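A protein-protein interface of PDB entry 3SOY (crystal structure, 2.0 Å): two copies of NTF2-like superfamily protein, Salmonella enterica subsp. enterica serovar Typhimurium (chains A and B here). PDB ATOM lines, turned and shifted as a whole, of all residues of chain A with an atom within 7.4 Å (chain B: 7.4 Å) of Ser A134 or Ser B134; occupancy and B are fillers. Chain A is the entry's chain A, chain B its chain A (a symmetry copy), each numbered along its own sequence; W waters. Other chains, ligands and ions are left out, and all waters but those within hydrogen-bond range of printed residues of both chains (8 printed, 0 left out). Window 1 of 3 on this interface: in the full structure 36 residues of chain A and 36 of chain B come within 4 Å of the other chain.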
ATOM      1  N   ILE A  44     -15.231 -20.194   6.053  1.00  0.00           N
ATOM      2  CA  ILE A  44     -15.814 -20.788   4.832  1.00  0.00           C
ATOM      3  C   ILE A  44     -14.898 -21.901   4.399  1.00  0.00           C
ATOM      4  O   ILE A  44     -13.704 -21.710   4.389  1.00  0.00           O
ATOM      5  CB  ILE A  44     -16.008 -19.805   3.703  1.00  0.00           C
ATOM      6  CG1 ILE A  44     -17.026 -18.749   4.107  1.00  0.00           C
ATOM      7  CG2 ILE A  44     -16.495 -20.495   2.440  1.00  0.00           C
ATOM      8  CD1 ILE A  44     -17.165 -17.573   3.117  1.00  0.00           C
ATOM      9  N   HIS A  45     -15.441 -23.097   4.147  1.00  0.00           N
ATOM     10  CA  HIS A  45     -14.594 -24.225   3.720  1.00  0.00           C
ATOM     11  C   HIS A  45     -15.335 -25.076   2.723  1.00  0.00           C
ATOM     12  O   HIS A  45     -16.493 -24.811   2.470  1.00  0.00           O
ATOM     13  CB  HIS A  45     -14.087 -25.027   4.917  1.00  0.00           C
ATOM     14  CG  HIS A  45     -15.158 -25.600   5.795  1.00  0.00           C
ATOM     15  ND1 HIS A  45     -15.560 -26.918   5.721  1.00  0.00           N
ATOM     16  CD2 HIS A  45     -15.873 -25.043   6.798  1.00  0.00           C
ATOM     17  CE1 HIS A  45     -16.489 -27.138   6.631  1.00  0.00           C
ATOM     18  NE2 HIS A  45     -16.702 -26.013   7.296  1.00  0.00           N
ATOM     19  N   PRO A  46     -14.673 -26.058   2.103  1.00  0.00           N
ATOM     20  CA  PRO A  46     -15.392 -26.774   1.030  1.00  0.00           C
ATOM     21  C   PRO A  46     -16.612 -27.576   1.470  1.00  0.00           C
ATOM     22  O   PRO A  46     -17.507 -27.826   0.648  1.00  0.00           O
ATOM     23  CB  PRO A  46     -14.304 -27.649   0.410  1.00  0.00           C
ATOM     24  CG  PRO A  46     -13.022 -26.837   0.700  1.00  0.00           C
ATOM     25  CD  PRO A  46     -13.239 -26.354   2.086  1.00  0.00           C
ATOM     26  N   GLY A  48     -18.738 -26.501   4.052  1.00  0.00           N
ATOM     27  CA  GLY A  48     -19.775 -25.657   4.656  1.00  0.00           C
ATOM     28  C   GLY A  48     -19.267 -24.310   5.068  1.00  0.00           C
ATOM     29  O   GLY A  48     -18.339 -23.812   4.487  1.00  0.00           O
ATOM     30  N   PHE A  93      -2.128 -18.226   1.748  1.00  0.00           N
ATOM     31  CA  PHE A  93      -1.124 -19.256   1.583  1.00  0.00           C
ATOM     32  C   PHE A  93      -1.631 -20.468   0.877  1.00  0.00           C
ATOM     33  O   PHE A  93      -2.817 -20.676   0.735  1.00  0.00           O
ATOM     34  CB  PHE A  93      -0.476 -19.660   2.925  1.00  0.00           C
ATOM     35  CG  PHE A  93      -1.436 -20.051   3.980  1.00  0.00           C
ATOM     36  CD1 PHE A  93      -1.911 -21.367   4.061  1.00  0.00           C
ATOM     37  CD2 PHE A  93      -1.837 -19.137   4.924  1.00  0.00           C
ATOM     38  CE1 PHE A  93      -2.779 -21.763   5.074  1.00  0.00           C
ATOM     39  CE2 PHE A  93      -2.683 -19.513   5.933  1.00  0.00           C
ATOM     40  CZ  PHE A  93      -3.181 -20.826   6.022  1.00  0.00           C
ATOM     41  N   TRP A  95      -1.339 -24.609   0.890  1.00  0.00           N
ATOM     42  CA  TRP A  95      -1.170 -25.601   1.922  1.00  0.00           C
ATOM     43  C   TRP A  95      -1.368 -27.003   1.364  1.00  0.00           C
ATOM     44  O   TRP A  95      -1.927 -27.213   0.259  1.00  0.00           O
ATOM     45  CB  TRP A  95      -2.179 -25.367   3.051  1.00  0.00           C
ATOM     46  CG  TRP A  95      -3.562 -25.299   2.580  1.00  0.00           C
ATOM     47  CD1 TRP A  95      -4.253 -24.165   2.215  1.00  0.00           C
ATOM     48  CD2 TRP A  95      -4.461 -26.411   2.373  1.00  0.00           C
ATOM     49  NE1 TRP A  95      -5.512 -24.505   1.793  1.00  0.00           N
ATOM     50  CE2 TRP A  95      -5.673 -25.873   1.879  1.00  0.00           C
ATOM     51  CE3 TRP A  95      -4.343 -27.806   2.520  1.00  0.00           C
ATOM     52  CZ2 TRP A  95      -6.776 -26.685   1.538  1.00  0.00           C
ATOM     53  CZ3 TRP A  95      -5.450 -28.613   2.199  1.00  0.00           C
ATOM     54  CH2 TRP A  95      -6.647 -28.049   1.705  1.00  0.00           C
ATOM     55  N   THR A 111      -4.792 -30.636  -1.038  1.00  0.00           N
ATOM     56  CA  THR A 111      -4.107 -29.342  -1.112  1.00  0.00           C
ATOM     57  C   THR A 111      -5.083 -28.203  -1.415  1.00  0.00           C
ATOM     58  O   THR A 111      -6.262 -28.425  -1.696  1.00  0.00           O
ATOM     59  CB  THR A 111      -3.027 -29.335  -2.188  1.00  0.00           C
ATOM     60  OG1 THR A 111      -3.666 -29.391  -3.472  1.00  0.00           O
ATOM     61  CG2 THR A 111      -2.093 -30.496  -2.022  1.00  0.00           C
ATOM     62  N   GLY A 112      -4.583 -26.973  -1.378  1.00  0.00           N
ATOM     63  CA  GLY A 112      -5.454 -25.857  -1.683  1.00  0.00           C
ATOM     64  C   GLY A 112      -4.869 -24.530  -1.299  1.00  0.00           C
ATOM     65  O   GLY A 112      -3.688 -24.422  -0.957  1.00  0.00           O
ATOM     66  N   ARG A 113      -5.714 -23.514  -1.380  1.00  0.00           N
ATOM     67  CA  ARG A 113      -5.359 -22.147  -1.030  1.00  0.00           C
ATOM     68  C   ARG A 113      -6.179 -21.739   0.148  1.00  0.00           C
ATOM     69  O   ARG A 113      -7.321 -22.146   0.265  1.00  0.00           O
ATOM     70  CB  ARG A 113      -5.711 -21.176  -2.170  1.00  0.00           C
ATOM     71  CG  ARG A 113      -4.783 -21.203  -3.381  1.00  0.00           C
ATOM     72  CD  ARG A 113      -5.066 -22.310  -4.403  1.00  0.00           C
ATOM     73  NE  ARG A 113      -6.473 -22.413  -4.759  1.00  0.00           N
ATOM     74  CZ  ARG A 113      -7.108 -21.713  -5.698  1.00  0.00           C
ATOM     75  NH1 ARG A 113      -6.467 -20.851  -6.500  1.00  0.00           N
ATOM     76  NH2 ARG A 113      -8.394 -21.940  -5.888  1.00  0.00           N
ATOM     77  N   GLU A 114      -5.617 -20.889   0.988  1.00  0.00           N
ATOM     78  CA  GLU A 114      -6.320 -20.368   2.161  1.00  0.00           C
ATOM     79  C   GLU A 114      -6.086 -18.867   2.337  1.00  0.00           C
ATOM     80  O   GLU A 114      -4.984 -18.376   2.167  1.00  0.00           O
ATOM     81  CB  GLU A 114      -5.827 -21.085   3.409  1.00  0.00           C
ATOM     82  CG  GLU A 114      -6.568 -20.689   4.734  1.00  0.00           C
ATOM     83  CD  GLU A 114      -6.505 -21.786   5.794  1.00  0.00           C
ATOM     84  OE1 GLU A 114      -6.488 -22.976   5.404  1.00  0.00           O
ATOM     85  OE2 GLU A 114      -6.532 -21.483   7.010  1.00  0.00           O
ATOM     86  N   SER A 115      -7.142 -18.151   2.678  1.00  0.00           N
ATOM     87  CA  SER A 115      -6.990 -16.772   3.134  1.00  0.00           C
ATOM     88  C   SER A 115      -7.535 -16.651   4.547  1.00  0.00           C
ATOM     89  O   SER A 115      -8.520 -17.253   4.880  1.00  0.00           O
ATOM     90  CB  SER A 115      -7.693 -15.728   2.268  1.00  0.00           C
ATOM     91  OG  SER A 115      -8.399 -16.209   1.177  1.00  0.00           O
ATOM     92  N   HIS A 132     -11.146 -18.410   4.701  1.00  0.00           N
ATOM     93  CA  HIS A 132     -11.831 -19.051   3.574  1.00  0.00           C
ATOM     94  C   HIS A 132     -10.816 -19.980   2.969  1.00  0.00           C
ATOM     95  O   HIS A 132      -9.739 -19.554   2.639  1.00  0.00           O
ATOM     96  CB  HIS A 132     -12.350 -17.970   2.634  1.00  0.00           C
ATOM     97  CG  HIS A 132     -13.210 -18.454   1.505  1.00  0.00           C
ATOM     98  ND1 HIS A 132     -14.164 -17.649   0.927  1.00  0.00           N
ATOM     99  CD2 HIS A 132     -13.210 -19.610   0.787  1.00  0.00           C
ATOM    100  CE1 HIS A 132     -14.733 -18.291  -0.090  1.00  0.00           C
ATOM    101  NE2 HIS A 132     -14.176 -19.489  -0.191  1.00  0.00           N
ATOM    102  N   TYR A 133     -11.095 -21.283   2.926  1.00  0.00           N
ATOM    103  CA  TYR A 133     -10.174 -22.133   2.192  1.00  0.00           C
ATOM    104  C   TYR A 133     -10.866 -22.914   1.095  1.00  0.00           C
ATOM    105  O   TYR A 133     -12.062 -23.126   1.128  1.00  0.00           O
ATOM    106  CB  TYR A 133      -9.279 -22.974   3.104  1.00  0.00           C
ATOM    107  CG  TYR A 133      -9.767 -24.308   3.637  1.00  0.00           C
ATOM    108  CD1 TYR A 133      -9.841 -25.425   2.837  1.00  0.00           C
ATOM    109  CD2 TYR A 133     -10.035 -24.471   4.975  1.00  0.00           C
ATOM    110  CE1 TYR A 133     -10.259 -26.661   3.339  1.00  0.00           C
ATOM    111  CE2 TYR A 133     -10.440 -25.707   5.483  1.00  0.00           C
ATOM    112  CZ  TYR A 133     -10.530 -26.799   4.667  1.00  0.00           C
ATOM    113  OH  TYR A 133     -10.930 -28.026   5.178  1.00  0.00           O
ATOM    114  N   SER A 134     -10.100 -23.196   0.050  1.00  0.00           N
ATOM    115  CA  SER A 134     -10.602 -23.905  -1.113  1.00  0.00           C
ATOM    116  C   SER A 134      -9.513 -24.801  -1.633  1.00  0.00           C
ATOM    117  O   SER A 134      -8.370 -24.713  -1.214  1.00  0.00           O
ATOM    118  CB  SER A 134     -11.112 -22.944  -2.227  1.00  0.00           C
ATOM    119  OG  SER A 134     -10.158 -22.002  -2.659  1.00  0.00           O
ATOM    120  N   GLY A 135      -9.889 -25.649  -2.569  1.00  0.00           N
ATOM    121  CA  GLY A 135      -8.962 -26.573  -3.174  1.00  0.00           C
ATOM    122  C   GLY A 135      -8.038 -25.887  -4.161  1.00  0.00           C
ATOM    123  O   GLY A 135      -8.083 -24.664  -4.328  1.00  0.00           O
ATOM    124  N   PRO A 136      -7.180 -26.681  -4.811  1.00  0.00           N
ATOM    125  CA  PRO A 136      -6.222 -26.124  -5.757  1.00  0.00           C
ATOM    126  C   PRO A 136      -6.928 -25.646  -7.008  1.00  0.00           C
ATOM    127  O   PRO A 136      -8.094 -26.017  -7.243  1.00  0.00           O
ATOM    128  CB  PRO A 136      -5.321 -27.320  -6.068  1.00  0.00           C
ATOM    129  CG  PRO A 136      -6.255 -28.518  -5.925  1.00  0.00           C
ATOM    130  CD  PRO A 136      -7.173 -28.169  -4.826  1.00  0.00           C
ATOM    131  N   ALA A 137      -6.232 -24.798  -7.765  1.00  0.00           N
ATOM    132  CA  ALA A 137      -6.757 -24.223  -8.983  1.00  0.00           C
ATOM    133  C   ALA A 137      -6.997 -25.345  -9.985  1.00  0.00           C
ATOM    134  O   ALA A 137      -6.281 -26.352  -9.983  1.00  0.00           O
ATOM    135  CB  ALA A 137      -5.804 -23.158  -9.554  1.00  0.00           C
ATOM    136  N   GLY A 144     -14.246 -24.414 -12.888  1.00  0.00           N
ATOM    137  CA  GLY A 144     -13.807 -23.406 -11.925  1.00  0.00           C
ATOM    138  C   GLY A 144     -14.481 -22.029 -11.992  1.00  0.00           C
ATOM    139  O   GLY A 144     -13.961 -21.052 -11.438  1.00  0.00           O
ATOM    140  N   TYR A 145     -15.650 -21.949 -12.611  1.00  0.00           N
ATOM    141  CA  TYR A 145     -16.403 -20.691 -12.642  1.00  0.00           C
ATOM    142  C   TYR A 145     -17.540 -20.738 -11.572  1.00  0.00           C
ATOM    143  O   TYR A 145     -17.560 -21.708 -10.795  1.00  0.00           O
ATOM    144  CB  TYR A 145     -16.946 -20.434 -14.050  1.00  0.00           C
ATOM    145  CG  TYR A 145     -15.891 -20.436 -15.144  1.00  0.00           C
ATOM    146  CD1 TYR A 145     -15.172 -19.286 -15.448  1.00  0.00           C
ATOM    147  CD2 TYR A 145     -15.643 -21.574 -15.897  1.00  0.00           C
ATOM    148  CE1 TYR A 145     -14.215 -19.268 -16.458  1.00  0.00           C
ATOM    149  CE2 TYR A 145     -14.669 -21.579 -16.905  1.00  0.00           C
ATOM    150  CZ  TYR A 145     -13.956 -20.419 -17.175  1.00  0.00           C
ATOM    151  OH  TYR A 145     -12.976 -20.417 -18.155  1.00  0.00           O
ATOM    152  OXT TYR A 145     -18.457 -19.861 -11.413  1.00  0.00           O
ATOM    153  N   ILE B  44      -8.285 -14.704  -5.049  1.00  0.00           N
ATOM    154  CA  ILE B  44      -8.164 -16.175  -5.137  1.00  0.00           C
ATOM    155  C   ILE B  44      -9.444 -16.690  -5.737  1.00  0.00           C
ATOM    156  O   ILE B  44     -10.499 -16.260  -5.333  1.00  0.00           O
ATOM    157  CB  ILE B  44      -7.901 -16.850  -3.812  1.00  0.00           C
ATOM    158  CG1 ILE B  44      -6.548 -16.412  -3.269  1.00  0.00           C
ATOM    159  CG2 ILE B  44      -7.906 -18.363  -3.948  1.00  0.00           C
ATOM    160  CD1 ILE B  44      -6.250 -16.876  -1.828  1.00  0.00           C
ATOM    161  N   HIS B  45      -9.355 -17.529  -6.775  1.00  0.00           N
ATOM    162  CA  HIS B  45     -10.574 -18.066  -7.405  1.00  0.00           C
ATOM    163  C   HIS B  45     -10.341 -19.486  -7.849  1.00  0.00           C
ATOM    164  O   HIS B  45      -9.230 -19.963  -7.731  1.00  0.00           O
ATOM    165  CB  HIS B  45     -11.059 -17.167  -8.541  1.00  0.00           C
ATOM    166  CG  HIS B  45     -10.067 -16.946  -9.641  1.00  0.00           C
ATOM    167  ND1 HIS B  45     -10.113 -17.631 -10.838  1.00  0.00           N
ATOM    168  CD2 HIS B  45      -9.034 -16.079  -9.742  1.00  0.00           C
ATOM    169  CE1 HIS B  45      -9.138 -17.205 -11.618  1.00  0.00           C
ATOM    170  NE2 HIS B  45      -8.464 -16.266 -10.973  1.00  0.00           N
ATOM    171  N   PRO B  46     -11.381 -20.194  -8.300  1.00  0.00           N
ATOM    172  CA  PRO B  46     -11.141 -21.623  -8.589  1.00  0.00           C
ATOM    173  C   PRO B  46     -10.166 -21.916  -9.724  1.00  0.00           C
ATOM    174  O   PRO B  46      -9.570 -23.004  -9.750  1.00  0.00           O
ATOM    175  CB  PRO B  46     -12.545 -22.159  -8.863  1.00  0.00           C
ATOM    176  CG  PRO B  46     -13.432 -21.205  -8.033  1.00  0.00           C
ATOM    177  CD  PRO B  46     -12.810 -19.879  -8.272  1.00  0.00           C
ATOM    178  N   GLY B  48      -7.351 -19.910 -10.351  1.00  0.00           N
ATOM    179  CA  GLY B  48      -6.008 -19.383 -10.085  1.00  0.00           C
ATOM    180  C   GLY B  48      -5.986 -18.358  -8.993  1.00  0.00           C
ATOM    181  O   GLY B  48      -6.810 -18.393  -8.118  1.00  0.00           O
ATOM    182  N   PHE B  93     -20.721 -13.690   1.148  1.00  0.00           N
ATOM    183  CA  PHE B  93     -22.006 -13.913   0.519  1.00  0.00           C
ATOM    184  C   PHE B  93     -22.044 -15.143  -0.324  1.00  0.00           C
ATOM    185  O   PHE B  93     -21.031 -15.711  -0.675  1.00  0.00           O
ATOM    186  CB  PHE B  93     -22.472 -12.694  -0.306  1.00  0.00           C
ATOM    187  CG  PHE B  93     -21.492 -12.215  -1.305  1.00  0.00           C
ATOM    188  CD1 PHE B  93     -21.438 -12.787  -2.584  1.00  0.00           C
ATOM    189  CD2 PHE B  93     -20.652 -11.169  -1.006  1.00  0.00           C
ATOM    190  CE1 PHE B  93     -20.554 -12.318  -3.551  1.00  0.00           C
ATOM    191  CE2 PHE B  93     -19.784 -10.690  -1.950  1.00  0.00           C
ATOM    192  CZ  PHE B  93     -19.707 -11.261  -3.234  1.00  0.00           C
ATOM    193  N   TRP B  95     -23.588 -16.604  -3.891  1.00  0.00           N
ATOM    194  CA  TRP B  95     -23.849 -16.024  -5.185  1.00  0.00           C
ATOM    195  C   TRP B  95     -24.205 -17.101  -6.200  1.00  0.00           C
ATOM    196  O   TRP B  95     -23.966 -18.317  -5.999  1.00  0.00           O
ATOM    197  CB  TRP B  95     -22.617 -15.260  -5.681  1.00  0.00           C
ATOM    198  CG  TRP B  95     -21.400 -16.072  -5.681  1.00  0.00           C
ATOM    199  CD1 TRP B  95     -20.479 -16.175  -4.662  1.00  0.00           C
ATOM    200  CD2 TRP B  95     -20.947 -16.948  -6.735  1.00  0.00           C
ATOM    201  NE1 TRP B  95     -19.494 -17.060  -5.017  1.00  0.00           N
ATOM    202  CE2 TRP B  95     -19.749 -17.550  -6.282  1.00  0.00           C
ATOM    203  CE3 TRP B  95     -21.456 -17.309  -7.997  1.00  0.00           C
ATOM    204  CZ2 TRP B  95     -19.038 -18.494  -7.055  1.00  0.00           C
ATOM    205  CZ3 TRP B  95     -20.737 -18.234  -8.775  1.00  0.00           C
ATOM    206  CH2 TRP B  95     -19.545 -18.822  -8.295  1.00  0.00           C
ATOM    207  N   THR B 111     -22.604 -21.623  -8.970  1.00  0.00           N
ATOM    208  CA  THR B 111     -22.859 -20.988  -7.673  1.00  0.00           C
ATOM    209  C   THR B 111     -21.658 -21.124  -6.734  1.00  0.00           C
ATOM    210  O   THR B 111     -20.684 -21.816  -7.032  1.00  0.00           O
ATOM    211  CB  THR B 111     -24.072 -21.593  -6.976  1.00  0.00           C
ATOM    212  OG1 THR B 111     -23.744 -22.933  -6.577  1.00  0.00           O
ATOM    213  CG2 THR B 111     -25.266 -21.599  -7.882  1.00  0.00           C
ATOM    214  N   GLY B 112     -21.738 -20.475  -5.579  1.00  0.00           N
ATOM    215  CA  GLY B 112     -20.643 -20.588  -4.637  1.00  0.00           C
ATOM    216  C   GLY B 112     -20.704 -19.572  -3.535  1.00  0.00           C
ATOM    217  O   GLY B 112     -21.704 -18.869  -3.363  1.00  0.00           O
ATOM    218  N   ARG B 113     -19.620 -19.520  -2.776  1.00  0.00           N
ATOM    219  CA  ARG B 113     -19.462 -18.590  -1.669  1.00  0.00           C
ATOM    220  C   ARG B 113     -18.342 -17.659  -1.998  1.00  0.00           C
ATOM    221  O   ARG B 113     -17.382 -18.061  -2.629  1.00  0.00           O
ATOM    222  CB  ARG B 113     -19.057 -19.327  -0.381  1.00  0.00           C
ATOM    223  CG  ARG B 113     -20.167 -20.110   0.316  1.00  0.00           C
ATOM    224  CD  ARG B 113     -20.444 -21.507  -0.251  1.00  0.00           C
ATOM    225  NE  ARG B 113     -19.234 -22.290  -0.457  1.00  0.00           N
ATOM    226  CZ  ARG B 113     -18.611 -23.042   0.450  1.00  0.00           C
ATOM    227  NH1 ARG B 113     -19.100 -23.220   1.686  1.00  0.00           N
ATOM    228  NH2 ARG B 113     -17.521 -23.689   0.085  1.00  0.00           N
ATOM    229  N   GLU B 114     -18.440 -16.432  -1.520  1.00  0.00           N
ATOM    230  CA  GLU B 114     -17.397 -15.427  -1.725  1.00  0.00           C
ATOM    231  C   GLU B 114     -17.118 -14.635  -0.447  1.00  0.00           C
ATOM    232  O   GLU B 114     -18.026 -14.259   0.273  1.00  0.00           O
ATOM    233  CB  GLU B 114     -17.833 -14.455  -2.812  1.00  0.00           C
ATOM    234  CG  GLU B 114     -16.762 -13.377  -3.201  1.00  0.00           C
ATOM    235  CD  GLU B 114     -16.951 -12.845  -4.620  1.00  0.00           C
ATOM    236  OE1 GLU B 114     -17.410 -13.629  -5.482  1.00  0.00           O
ATOM    237  OE2 GLU B 114     -16.595 -11.677  -4.902  1.00  0.00           O
ATOM    238  N   SER B 115     -15.847 -14.393  -0.179  1.00  0.00           N
ATOM    239  CA  SER B 115     -15.476 -13.427   0.852  1.00  0.00           C
ATOM    240  C   SER B 115     -14.655 -12.315   0.221  1.00  0.00           C
ATOM    241  O   SER B 115     -13.858 -12.554  -0.646  1.00  0.00           O
ATOM    242  CB  SER B 115     -14.669 -14.007   2.012  1.00  0.00           C
ATOM    243  OG  SER B 115     -14.373 -15.358   1.940  1.00  0.00           O
ATOM    244  N   HIS B 132     -11.804 -13.956  -2.090  1.00  0.00           N
ATOM    245  CA  HIS B 132     -11.584 -15.392  -2.281  1.00  0.00           C
ATOM    246  C   HIS B 132     -12.933 -15.959  -2.624  1.00  0.00           C
ATOM    247  O   HIS B 132     -13.868 -15.755  -1.894  1.00  0.00           O
ATOM    248  CB  HIS B 132     -10.951 -15.966  -1.019  1.00  0.00           C
ATOM    249  CG  HIS B 132     -10.520 -17.399  -1.106  1.00  0.00           C
ATOM    250  ND1 HIS B 132      -9.496 -17.894  -0.331  1.00  0.00           N
ATOM    251  CD2 HIS B 132     -11.015 -18.462  -1.796  1.00  0.00           C
ATOM    252  CE1 HIS B 132      -9.362 -19.200  -0.550  1.00  0.00           C
ATOM    253  NE2 HIS B 132     -10.269 -19.568  -1.443  1.00  0.00           N
ATOM    254  N   TYR B 133     -13.082 -16.573  -3.797  1.00  0.00           N
ATOM    255  CA  TYR B 133     -14.344 -17.252  -4.033  1.00  0.00           C
ATOM    256  C   TYR B 133     -14.155 -18.717  -4.361  1.00  0.00           C
ATOM    257  O   TYR B 133     -13.100 -19.137  -4.795  1.00  0.00           O
ATOM    258  CB  TYR B 133     -15.259 -16.497  -5.000  1.00  0.00           C
ATOM    259  CG  TYR B 133     -15.111 -16.685  -6.498  1.00  0.00           C
ATOM    260  CD1 TYR B 133     -15.543 -17.827  -7.132  1.00  0.00           C
ATOM    261  CD2 TYR B 133     -14.650 -15.659  -7.289  1.00  0.00           C
ATOM    262  CE1 TYR B 133     -15.436 -17.984  -8.517  1.00  0.00           C
ATOM    263  CE2 TYR B 133     -14.554 -15.806  -8.675  1.00  0.00           C
ATOM    264  CZ  TYR B 133     -14.966 -16.958  -9.282  1.00  0.00           C
ATOM    265  OH  TYR B 133     -14.872 -17.097 -10.660  1.00  0.00           O
ATOM    266  N   SER B 134     -15.160 -19.500  -3.993  1.00  0.00           N
ATOM    267  CA  SER B 134     -15.137 -20.939  -4.192  1.00  0.00           C
ATOM    268  C   SER B 134     -16.528 -21.396  -4.530  1.00  0.00           C
ATOM    269  O   SER B 134     -17.484 -20.644  -4.416  1.00  0.00           O
ATOM    270  CB  SER B 134     -14.584 -21.706  -2.955  1.00  0.00           C
ATOM    271  OG  SER B 134     -15.267 -21.435  -1.753  1.00  0.00           O
ATOM    272  N   GLY B 135     -16.622 -22.648  -4.927  1.00  0.00           N
ATOM    273  CA  GLY B 135     -17.888 -23.240  -5.283  1.00  0.00           C
ATOM    274  C   GLY B 135     -18.729 -23.559  -4.063  1.00  0.00           C
ATOM    275  O   GLY B 135     -18.344 -23.257  -2.929  1.00  0.00           O
ATOM    276  N   PRO B 136     -19.900 -24.163  -4.299  1.00  0.00           N
ATOM    277  CA  PRO B 136     -20.805 -24.484  -3.204  1.00  0.00           C
ATOM    278  C   PRO B 136     -20.245 -25.614  -2.367  1.00  0.00           C
ATOM    279  O   PRO B 136     -19.320 -26.318  -2.814  1.00  0.00           O
ATOM    280  CB  PRO B 136     -22.073 -24.929  -3.934  1.00  0.00           C
ATOM    281  CG  PRO B 136     -21.544 -25.544  -5.227  1.00  0.00           C
ATOM    282  CD  PRO B 136     -20.367 -24.734  -5.591  1.00  0.00           C
ATOM    283  N   ALA B 137     -20.780 -25.741  -1.152  1.00  0.00           N
ATOM    284  CA  ALA B 137     -20.352 -26.750  -0.209  1.00  0.00           C
ATOM    285  C   ALA B 137     -20.669 -28.122  -0.790  1.00  0.00           C
ATOM    286  O   ALA B 137     -21.646 -28.280  -1.531  1.00  0.00           O
ATOM    287  CB  ALA B 137     -21.023 -26.554   1.162  1.00  0.00           C
ATOM    288  N   GLY B 144     -14.200 -32.538  -0.098  1.00  0.00           N
ATOM    289  CA  GLY B 144     -14.110 -31.182   0.440  1.00  0.00           C
ATOM    290  C   GLY B 144     -13.072 -30.929   1.540  1.00  0.00           C
ATOM    291  O   GLY B 144     -13.147 -29.916   2.249  1.00  0.00           O
ATOM    292  N   TYR B 145     -12.079 -31.799   1.658  1.00  0.00           N
ATOM    293  CA  TYR B 145     -10.996 -31.583   2.624  1.00  0.00           C
ATOM    294  C   TYR B 145      -9.743 -31.017   1.884  1.00  0.00           C
ATOM    295  O   TYR B 145      -9.872 -30.709   0.686  1.00  0.00           O
ATOM    296  CB  TYR B 145     -10.687 -32.884   3.370  1.00  0.00           C
ATOM    297  CG  TYR B 145     -11.883 -33.516   4.062  1.00  0.00           C
ATOM    298  CD1 TYR B 145     -12.259 -33.126   5.343  1.00  0.00           C
ATOM    299  CD2 TYR B 145     -12.612 -34.526   3.452  1.00  0.00           C
ATOM    300  CE1 TYR B 145     -13.342 -33.706   5.995  1.00  0.00           C
ATOM    301  CE2 TYR B 145     -13.718 -35.109   4.087  1.00  0.00           C
ATOM    302  CZ  TYR B 145     -14.077 -34.688   5.360  1.00  0.00           C
ATOM    303  OH  TYR B 145     -15.180 -35.241   5.990  1.00  0.00           O
ATOM    304  OXT TYR B 145      -8.589 -30.830   2.400  1.00  0.00           O
HETATM  305  O   HOH W   1     -14.570 -23.639  -0.160  1.00  0.00           O
HETATM  306  O   HOH W   2      -8.725 -29.891   4.943  1.00  0.00           O
HETATM  307  O   HOH W   3     -11.174 -21.227  -5.158  1.00  0.00           O
HETATM  308  O   HOH W   4     -16.834 -26.809  -2.055  1.00  0.00           O
HETATM  309  O   HOH W   5     -10.411 -24.775  -7.525  1.00  0.00           O
HETATM  310  O   HOH W   6     -17.545 -17.328 -11.754  1.00  0.00           O
HETATM  311  O   HOH W   7     -12.742 -18.473 -11.603  1.00  0.00           O
HETATM  312  O   HOH W   8     -13.520 -28.713   4.813  1.00  0.00           O
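Of chain B, only His B132 (2.7 Å) and Ser B134 (3.8 Å) come within 4 Å of Ser A134.
No residue of chain B comes within 4 Å of Gly A135.
No residue of chain A comes within 4 Å of Gly B135.
Printed residues of chain A within 4 Å of Trp B95: Tyr A145.
Printed residues of chain B within 4 Å of Ile A44: Arg B113 and Ser B115.
Thr A111 touches none of the printed residues of chain B.
The nearest residue of chain B that does not touch Ser A134 is Ile B44 (4.5 Å).
The nearest residue of chain A that does not touch Ser B134 is Ile A44 (4.5 Å).
The nearest printed residue of chain A that does not touch Trp B95 is Gly A144 (6.8 Å).
O of His A45 lies within hydrogen-bond range of NH2 of Arg B113 (2.8 Å).
The backbone carbonyl oxygen (O) of Gly A48 lies within hydrogen-bond range of the guanidinium group (NH1) of Arg B113 (3.0 Å).
The backbone carbonyl oxygen (O) of His B45 sits at hydrogen-bond distance from the guanidinium group (NH2) of Arg A113, 2.8 Å away.
The guanidinium group (NH1) of Arg A113 lies within hydrogen-bond range of the backbone carbonyl oxygen (O) of Gly B48 (3.0 Å).
The side-chain hydroxyl (OG) of Ser A115 sits at hydrogen-bond distance from a ring nitrogen (ND1) of His B132 (2.5 Å).
ND1 of His A132 is in hydrogen-bond range of OG of Ser B115 (2.5 Å).
A ring nitrogen (ND1) of His A132 lies close to the backbone carbonyl oxygen of His B132 (3.4 Å).
NE2 of His A132 is in hydrogen-bond range of OG of Ser B134 (2.7 Å).
NE2 of His B132 lies within hydrogen-bond range of OG of Ser A134 (2.7 Å).
Water W3 lies within hydrogen-bond range of OG of Ser A134 (2.8 Å), O of Tyr B133 (2.9 Å), NH2 of Arg A113 (3.0 Å) and O of His B45 (3.5 Å).
Of the 19 printed residues of chain B, 12 touch a printed residue of chain A.
Of the 19 printed residues of chain A, 12 touch a printed residue of chain B.
Along chain A the printed residues that touch a printed residue of chain B span positions 44 to 145.
Among the printed residues, 26 pairs touch across the chains.
NE1 of Trp A95 sits close to O of Arg A113.
The backbone carbonyl oxygen (O) of Ile B44 is in hydrogen-bond range of the backbone NH (N) of Tyr B133, at 3.0 Å.
Ser A115 touches His B132, and with the chains exchanged His A132 touches Ser B115.
Positions printed for both chains: 44, 45, 46, 48, 93, 95, 111, 112, 113, 114, 115, 132, 133, 134, 135, 136, 137, 144 and 145.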
